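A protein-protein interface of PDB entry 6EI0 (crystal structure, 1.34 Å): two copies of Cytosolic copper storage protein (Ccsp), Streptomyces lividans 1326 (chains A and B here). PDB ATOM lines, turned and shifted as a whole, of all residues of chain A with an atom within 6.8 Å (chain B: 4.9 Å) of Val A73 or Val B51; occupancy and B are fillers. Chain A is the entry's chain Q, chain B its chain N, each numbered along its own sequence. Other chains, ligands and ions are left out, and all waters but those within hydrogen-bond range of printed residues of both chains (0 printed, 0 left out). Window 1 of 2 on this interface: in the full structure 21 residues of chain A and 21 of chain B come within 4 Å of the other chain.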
ATOM      1  N   VAL A  51     -21.336   7.379  25.988  1.00  0.00           N
ATOM      2  CA  VAL A  51     -20.522   8.066  24.996  1.00  0.00           C
ATOM      3  C   VAL A  51     -21.397   8.972  24.123  1.00  0.00           C
ATOM      4  O   VAL A  51     -20.983  10.079  23.776  1.00  0.00           O
ATOM      5  CB  VAL A  51     -19.704   7.101  24.162  1.00  0.00           C
ATOM      6  CG1 VAL A  51     -18.983   7.834  23.033  1.00  0.00           C
ATOM      7  CG2 VAL A  51     -18.670   6.407  25.059  1.00  0.00           C
ATOM      8  N   ALA A  54     -22.212  12.291  25.942  1.00  0.00           N
ATOM      9  CA  ALA A  54     -20.964  13.077  26.011  1.00  0.00           C
ATOM     10  C   ALA A  54     -20.649  13.713  24.662  1.00  0.00           C
ATOM     11  O   ALA A  54     -20.220  14.874  24.594  1.00  0.00           O
ATOM     12  CB  ALA A  54     -19.776  12.271  26.516  1.00  0.00           C
ATOM     13  N   THR A  55     -20.839  12.922  23.602  1.00  0.00           N
ATOM     14  CA  THR A  55     -20.553  13.381  22.261  1.00  0.00           C
ATOM     15  C   THR A  55     -21.504  14.545  21.890  1.00  0.00           C
ATOM     16  O   THR A  55     -21.082  15.548  21.348  1.00  0.00           O
ATOM     17  CB  THR A  55     -20.627  12.212  21.252  1.00  0.00           C
ATOM     18  OG1 THR A  55     -19.631  11.232  21.598  1.00  0.00           O
ATOM     19  CG2 THR A  55     -20.384  12.631  19.823  1.00  0.00           C
ATOM     20  N   ALA A  56     -22.797  14.362  22.176  1.00  0.00           N
ATOM     21  CA  ALA A  56     -23.763  15.461  21.917  1.00  0.00           C
ATOM     22  C   ALA A  56     -23.327  16.726  22.632  1.00  0.00           C
ATOM     23  O   ALA A  56     -23.408  17.827  22.054  1.00  0.00           O
ATOM     24  CB  ALA A  56     -25.119  15.029  22.373  1.00  0.00           C
ATOM     25  N   VAL A  58     -20.222  17.639  23.666  1.00  0.00           N
ATOM     26  CA  VAL A  58     -19.010  18.206  23.066  1.00  0.00           C
ATOM     27  C   VAL A  58     -19.372  18.934  21.751  1.00  0.00           C
ATOM     28  O   VAL A  58     -18.873  20.022  21.479  1.00  0.00           O
ATOM     29  CB  VAL A  58     -17.926  17.119  22.877  1.00  0.00           C
ATOM     30  CG1 VAL A  58     -16.779  17.651  22.008  1.00  0.00           C
ATOM     31  CG2 VAL A  58     -17.385  16.694  24.246  1.00  0.00           C
ATOM     32  N   LEU A  59     -20.215  18.326  20.934  1.00  0.00           N
ATOM     33  CA  LEU A  59     -20.568  18.910  19.661  1.00  0.00           C
ATOM     34  C   LEU A  59     -21.383  20.207  19.804  1.00  0.00           C
ATOM     35  O   LEU A  59     -21.454  20.976  18.856  1.00  0.00           O
ATOM     36  CB  LEU A  59     -21.405  17.932  18.812  1.00  0.00           C
ATOM     37  CG  LEU A  59     -20.666  16.690  18.242  1.00  0.00           C
ATOM     38  CD1 LEU A  59     -21.655  15.753  17.612  1.00  0.00           C
ATOM     39  CD2 LEU A  59     -19.622  17.161  17.254  1.00  0.00           C
ATOM     40  N   ASN A  68      -9.188  18.705  16.831  1.00  0.00           N
ATOM     41  CA  ASN A  68      -8.571  17.436  17.240  1.00  0.00           C
ATOM     42  C   ASN A  68      -9.350  16.747  18.373  1.00  0.00           C
ATOM     43  O   ASN A  68      -9.489  15.511  18.408  1.00  0.00           O
ATOM     44  CB  ASN A  68      -7.096  17.611  17.677  1.00  0.00           C
ATOM     45  CG  ASN A  68      -6.173  17.929  16.531  1.00  0.00           C
ATOM     46  OD1 ASN A  68      -6.465  17.670  15.364  1.00  0.00           O
ATOM     47  ND2 ASN A  68      -5.025  18.482  16.869  1.00  0.00           N
ATOM     48  N   VAL A  69      -9.801  17.535  19.334  1.00  0.00           N
ATOM     49  CA  VAL A  69     -10.616  16.995  20.409  1.00  0.00           C
ATOM     50  C   VAL A  69     -11.931  16.458  19.888  1.00  0.00           C
ATOM     51  O   VAL A  69     -12.314  15.346  20.209  1.00  0.00           O
ATOM     52  CB  VAL A  69     -10.885  18.047  21.487  1.00  0.00           C
ATOM     53  CG1 VAL A  69     -11.946  17.596  22.473  1.00  0.00           C
ATOM     54  CG2 VAL A  69      -9.595  18.384  22.227  1.00  0.00           C
ATOM     55  N   THR A  70     -12.612  17.270  19.090  1.00  0.00           N
ATOM     56  CA  THR A  70     -13.894  16.910  18.572  1.00  0.00           C
ATOM     57  C   THR A  70     -13.800  15.643  17.729  1.00  0.00           C
ATOM     58  O   THR A  70     -14.626  14.759  17.877  1.00  0.00           O
ATOM     59  CB  THR A  70     -14.484  18.119  17.842  1.00  0.00           C
ATOM     60  OG1 THR A  70     -14.686  19.176  18.793  1.00  0.00           O
ATOM     61  CG2 THR A  70     -15.752  17.734  17.124  1.00  0.00           C
ATOM     62  N   ARG A  71     -12.768  15.552  16.879  1.00  0.00           N
ATOM     63  CA  ARG A  71     -12.556  14.341  16.084  1.00  0.00           C
ATOM     64  C   ARG A  71     -12.341  13.098  16.944  1.00  0.00           C
ATOM     65  O   ARG A  71     -12.903  12.048  16.667  1.00  0.00           O
ATOM     66  CB  ARG A  71     -11.392  14.547  15.111  1.00  0.00           C
ATOM     67  CG  ARG A  71     -11.760  15.493  13.966  1.00  0.00           C
ATOM     68  CD  ARG A  71     -10.641  15.550  12.936  1.00  0.00           C
ATOM     69  NE  ARG A  71     -10.655  14.323  12.154  1.00  0.00           N
ATOM     70  CZ  ARG A  71     -11.472  14.086  11.115  1.00  0.00           C
ATOM     71  NH1 ARG A  71     -12.334  15.013  10.676  1.00  0.00           N
ATOM     72  NH2 ARG A  71     -11.405  12.912  10.495  1.00  0.00           N
ATOM     73  N   ALA A  72     -11.533  13.232  17.987  1.00  0.00           N
ATOM     74  CA  ALA A  72     -11.294  12.081  18.873  1.00  0.00           C
ATOM     75  C   ALA A  72     -12.572  11.569  19.553  1.00  0.00           C
ATOM     76  O   ALA A  72     -12.780  10.351  19.687  1.00  0.00           O
ATOM     77  CB  ALA A  72     -10.192  12.366  19.921  1.00  0.00           C
ATOM     78  N   VAL A  73     -13.440  12.505  19.940  1.00  0.00           N
ATOM     79  CA  VAL A  73     -14.705  12.177  20.565  1.00  0.00           C
ATOM     80  C   VAL A  73     -15.621  11.504  19.551  1.00  0.00           C
ATOM     81  O   VAL A  73     -16.232  10.477  19.852  1.00  0.00           O
ATOM     82  CB  VAL A  73     -15.330  13.394  21.266  1.00  0.00           C
ATOM     83  CG1 VAL A  73     -16.694  13.034  21.827  1.00  0.00           C
ATOM     84  CG2 VAL A  73     -14.411  13.864  22.378  1.00  0.00           C
ATOM     85  N   LEU A  74     -15.705  12.081  18.352  1.00  0.00           N
ATOM     86  CA  LEU A  74     -16.511  11.494  17.283  1.00  0.00           C
ATOM     87  C   LEU A  74     -16.042  10.072  16.940  1.00  0.00           C
ATOM     88  O   LEU A  74     -16.876   9.196  16.650  1.00  0.00           O
ATOM     89  CB  LEU A  74     -16.478  12.357  16.037  1.00  0.00           C
ATOM     90  CG  LEU A  74     -17.347  13.602  16.138  1.00  0.00           C
ATOM     91  CD1 LEU A  74     -16.914  14.546  15.026  1.00  0.00           C
ATOM     92  CD2 LEU A  74     -18.805  13.200  15.997  1.00  0.00           C
ATOM     93  N   GLN A  75     -14.711   9.856  16.936  1.00  0.00           N
ATOM     94  CA  GLN A  75     -14.179   8.533  16.650  1.00  0.00           C
ATOM     95  C   GLN A  75     -14.602   7.532  17.714  1.00  0.00           C
ATOM     96  O   GLN A  75     -14.991   6.408  17.380  1.00  0.00           O
ATOM     97  CB  GLN A  75     -12.647   8.550  16.466  1.00  0.00           C
ATOM     98  CG  GLN A  75     -12.113   7.198  15.952  1.00  0.00           C
ATOM     99  CD  GLN A  75     -12.768   6.806  14.609  1.00  0.00           C
ATOM    100  OE1 GLN A  75     -12.521   7.445  13.575  1.00  0.00           O
ATOM    101  NE2 GLN A  75     -13.647   5.785  14.635  1.00  0.00           N
ATOM    102  N   ALA A  76     -14.560   7.942  18.976  1.00  0.00           N
ATOM    103  CA  ALA A  76     -15.039   7.088  20.044  1.00  0.00           C
ATOM    104  C   ALA A  76     -16.528   6.769  19.838  1.00  0.00           C
ATOM    105  O   ALA A  76     -16.938   5.636  19.984  1.00  0.00           O
ATOM    106  CB  ALA A  76     -14.777   7.685  21.401  1.00  0.00           C
ATOM    107  N   CYS A  77     -17.345   7.792  19.552  1.00  0.00           N
ATOM    108  CA  CYS A  77     -18.778   7.569  19.398  1.00  0.00           C
ATOM    109  C   CYS A  77     -19.074   6.625  18.225  1.00  0.00           C
ATOM    110  O   CYS A  77     -19.893   5.693  18.367  1.00  0.00           O
ATOM    111  CB  CYS A  77     -19.486   8.904  19.247  1.00  0.00           C
ATOM    112  SG  CYS A  77     -21.247   8.805  19.560  1.00  0.00           S
ATOM    113  N   ALA A  78     -18.377   6.832  17.102  1.00  0.00           N
ATOM    114  CA  ALA A  78     -18.580   5.948  15.948  1.00  0.00           C
ATOM    115  C   ALA A  78     -18.241   4.493  16.316  1.00  0.00           C
ATOM    116  O   ALA A  78     -18.970   3.566  15.983  1.00  0.00           O
ATOM    117  CB  ALA A  78     -17.746   6.398  14.775  1.00  0.00           C
ATOM    118  N   CYS A 112     -21.945  10.272  12.891  1.00  0.00           N
ATOM    119  CA  CYS A 112     -20.602  10.541  13.392  1.00  0.00           C
ATOM    120  C   CYS A 112     -19.568  10.405  12.286  1.00  0.00           C
ATOM    121  O   CYS A 112     -18.656  11.226  12.160  1.00  0.00           O
ATOM    122  CB  CYS A 112     -20.249   9.569  14.536  1.00  0.00           C
ATOM    123  SG  CYS A 112     -21.139   9.827  16.063  1.00  0.00           S
ATOM    124  N   LEU A 116     -16.697  12.987  10.733  1.00  0.00           N
ATOM    125  CA  LEU A 116     -15.293  12.608  10.609  1.00  0.00           C
ATOM    126  C   LEU A 116     -14.793  12.795   9.177  1.00  0.00           C
ATOM    127  O   LEU A 116     -13.654  13.198   8.975  1.00  0.00           O
ATOM    128  CB  LEU A 116     -15.096  11.162  11.083  1.00  0.00           C
ATOM    129  CG  LEU A 116     -15.229  10.967  12.583  1.00  0.00           C
ATOM    130  CD1 LEU A 116     -15.461   9.523  12.975  1.00  0.00           C
ATOM    131  CD2 LEU A 116     -14.025  11.528  13.331  1.00  0.00           C
ATOM    132  N   ASP B  47     -15.546  19.967  28.272  1.00  0.00           N
ATOM    133  CA  ASP B  47     -15.345  18.794  27.438  1.00  0.00           C
ATOM    134  C   ASP B  47     -14.624  17.655  28.206  1.00  0.00           C
ATOM    135  O   ASP B  47     -15.024  16.496  28.136  1.00  0.00           O
ATOM    136  CB  ASP B  47     -14.505  19.135  26.225  1.00  0.00           C
ATOM    137  CG  ASP B  47     -15.231  19.908  25.138  1.00  0.00           C
ATOM    138  OD1 ASP B  47     -16.465  20.009  25.149  1.00  0.00           O
ATOM    139  OD2 ASP B  47     -14.497  20.395  24.256  1.00  0.00           O
ATOM    140  N   CYS B  48     -13.573  18.030  28.945  1.00  0.00           N
ATOM    141  CA  CYS B  48     -12.759  16.998  29.621  1.00  0.00           C
ATOM    142  C   CYS B  48     -13.586  16.318  30.685  1.00  0.00           C
ATOM    143  O   CYS B  48     -13.624  15.101  30.794  1.00  0.00           O
ATOM    144  CB  CYS B  48     -11.576  17.701  30.196  1.00  0.00           C
ATOM    145  SG  CYS B  48     -10.292  16.514  30.700  1.00  0.00           S
ATOM    146  N   ALA B  49     -14.435  17.074  31.399  1.00  0.00           N
ATOM    147  CA  ALA B  49     -15.274  16.477  32.388  1.00  0.00           C
ATOM    148  C   ALA B  49     -16.267  15.493  31.772  1.00  0.00           C
ATOM    149  O   ALA B  49     -16.464  14.399  32.276  1.00  0.00           O
ATOM    150  CB  ALA B  49     -15.964  17.542  33.211  1.00  0.00           C
ATOM    151  N   ASP B  50     -16.861  15.888  30.647  1.00  0.00           N
ATOM    152  CA  ASP B  50     -17.820  15.011  29.997  1.00  0.00           C
ATOM    153  C   ASP B  50     -17.172  13.706  29.494  1.00  0.00           C
ATOM    154  O   ASP B  50     -17.721  12.621  29.643  1.00  0.00           O
ATOM    155  CB  ASP B  50     -18.522  15.722  28.846  1.00  0.00           C
ATOM    156  CG  ASP B  50     -19.542  16.776  29.328  1.00  0.00           C
ATOM    157  OD1 ASP B  50     -20.071  16.673  30.489  1.00  0.00           O
ATOM    158  OD2 ASP B  50     -19.752  17.679  28.506  1.00  0.00           O
ATOM    159  N   VAL B  51     -15.990  13.862  28.894  1.00  0.00           N
ATOM    160  CA  VAL B  51     -15.328  12.667  28.328  1.00  0.00           C
ATOM    161  C   VAL B  51     -14.730  11.760  29.434  1.00  0.00           C
ATOM    162  O   VAL B  51     -14.929  10.548  29.368  1.00  0.00           O
ATOM    163  CB  VAL B  51     -14.271  13.099  27.325  1.00  0.00           C
ATOM    164  CG1 VAL B  51     -13.432  11.895  26.862  1.00  0.00           C
ATOM    165  CG2 VAL B  51     -14.890  13.774  26.124  1.00  0.00           C
ATOM    166  N   CYS B  52     -14.177  12.361  30.472  1.00  0.00           N
ATOM    167  CA  CYS B  52     -13.732  11.602  31.645  1.00  0.00           C
ATOM    168  C   CYS B  52     -14.867  10.865  32.300  1.00  0.00           C
ATOM    169  O   CYS B  52     -14.713   9.738  32.781  1.00  0.00           O
ATOM    170  CB  CYS B  52     -13.023  12.465  32.648  1.00  0.00           C
ATOM    171  SG  CYS B  52     -11.361  12.992  32.199  1.00  0.00           S
ATOM    172  N   THR B  53     -16.055  11.509  32.363  1.00  0.00           N
ATOM    173  CA  THR B  53     -17.201  10.888  32.976  1.00  0.00           C
ATOM    174  C   THR B  53     -17.622   9.627  32.201  1.00  0.00           C
ATOM    175  O   THR B  53     -17.891   8.572  32.802  1.00  0.00           O
ATOM    176  CB  THR B  53     -18.365  11.917  33.100  1.00  0.00           C
ATOM    177  OG1 THR B  53     -17.985  12.878  34.050  1.00  0.00           O
ATOM    178  CG2 THR B  53     -19.663  11.305  33.539  1.00  0.00           C
ATOM    179  N   ALA B  54     -17.704   9.742  30.879  1.00  0.00           N
ATOM    180  CA  ALA B  54     -18.041   8.622  30.011  1.00  0.00           C
ATOM    181  C   ALA B  54     -16.972   7.508  30.110  1.00  0.00           C
ATOM    182  O   ALA B  54     -17.327   6.354  30.214  1.00  0.00           O
ATOM    183  CB  ALA B  54     -18.159   9.049  28.573  1.00  0.00           C
ATOM    184  N   THR B  55     -15.718   7.936  30.153  1.00  0.00           N
ATOM    185  CA  THR B  55     -14.575   6.958  30.144  1.00  0.00           C
ATOM    186  C   THR B  55     -14.585   6.171  31.448  1.00  0.00           C
ATOM    187  O   THR B  55     -14.395   4.945  31.424  1.00  0.00           O
ATOM    188  CB  THR B  55     -13.262   7.708  29.940  1.00  0.00           C
ATOM    189  OG1 THR B  55     -13.269   8.411  28.696  1.00  0.00           O
ATOM    190  CG2 THR B  55     -12.033   6.731  29.927  1.00  0.00           C
ATOM    191  N   ALA B  76      -9.827   9.015  23.214  1.00  0.00           N
ATOM    192  CA  ALA B  76     -10.562  10.292  23.310  1.00  0.00           C
ATOM    193  C   ALA B  76     -10.228  10.960  24.647  1.00  0.00           C
ATOM    194  O   ALA B  76      -9.985  12.169  24.690  1.00  0.00           O
ATOM    195  CB  ALA B  76     -12.048  10.058  23.172  1.00  0.00           C
ATOM    196  N   CYS B  77     -10.192  10.171  25.724  1.00  0.00           N
ATOM    197  CA  CYS B  77      -9.920  10.719  27.028  1.00  0.00           C
ATOM    198  C   CYS B  77      -8.512  11.299  27.089  1.00  0.00           C
ATOM    199  O   CYS B  77      -8.286  12.399  27.560  1.00  0.00           O
ATOM    200  CB  CYS B  77     -10.173   9.704  28.099  1.00  0.00           C
ATOM    201  SG  CYS B  77     -10.414  10.370  29.743  1.00  0.00           S
ATOM    202  N   VAL B  80      -8.378  14.649  25.071  1.00  0.00           N
ATOM    203  CA  VAL B  80      -8.962  15.846  25.686  1.00  0.00           C
ATOM    204  C   VAL B  80      -8.265  16.205  26.992  1.00  0.00           C
ATOM    205  O   VAL B  80      -8.113  17.390  27.274  1.00  0.00           O
ATOM    206  CB  VAL B  80     -10.482  15.733  25.866  1.00  0.00           C
ATOM    207  CG1 VAL B  80     -10.838  14.705  26.931  1.00  0.00           C
ATOM    208  CG2 VAL B  80     -11.103  17.113  26.211  1.00  0.00           C
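The backbone carbonyl oxygen (O) of Val B51 lies within hydrogen-bond range of the side-chain hydroxyl (OG1) of Thr B55.
Among the printed residues, merely in contact across the chains: Ala A54 with Asp B50, Val A58 with Asp B47, Val A69 with Val B80, Ala A72 with Ala B76 and Val A73 with Val B51.
Val A73 touches just one residue of chain B: Val B51.
Val B51 touches just one residue of chain A: Val A73 (3.8 Å).
Printed residues of chain A within 4 Å of Asp B47: Val A58 (3.6 Å).
Of the printed residues of chain B, Val A69 touches Val B80.
Of the printed residues of chain A, Ala B76 touches Ala A72.
Cys B52 touches none of the printed residues of chain A.
The nearest printed residue of chain B that does not touch Val A73 is Ala B76 (4.3 Å).
Hydrophobic or aromatic side chains of chain A within 4 Å of the printed part of chain B: Ala A54, Val A58, Val A69, Ala A72 and Val A73.
Among the printed residues, 5 pairs touch across the chains.
5 positions are printed for both chains.
Of the 5 pairs that touch across the chains among the printed residues, none has its exchanged pair printed and touching as well.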
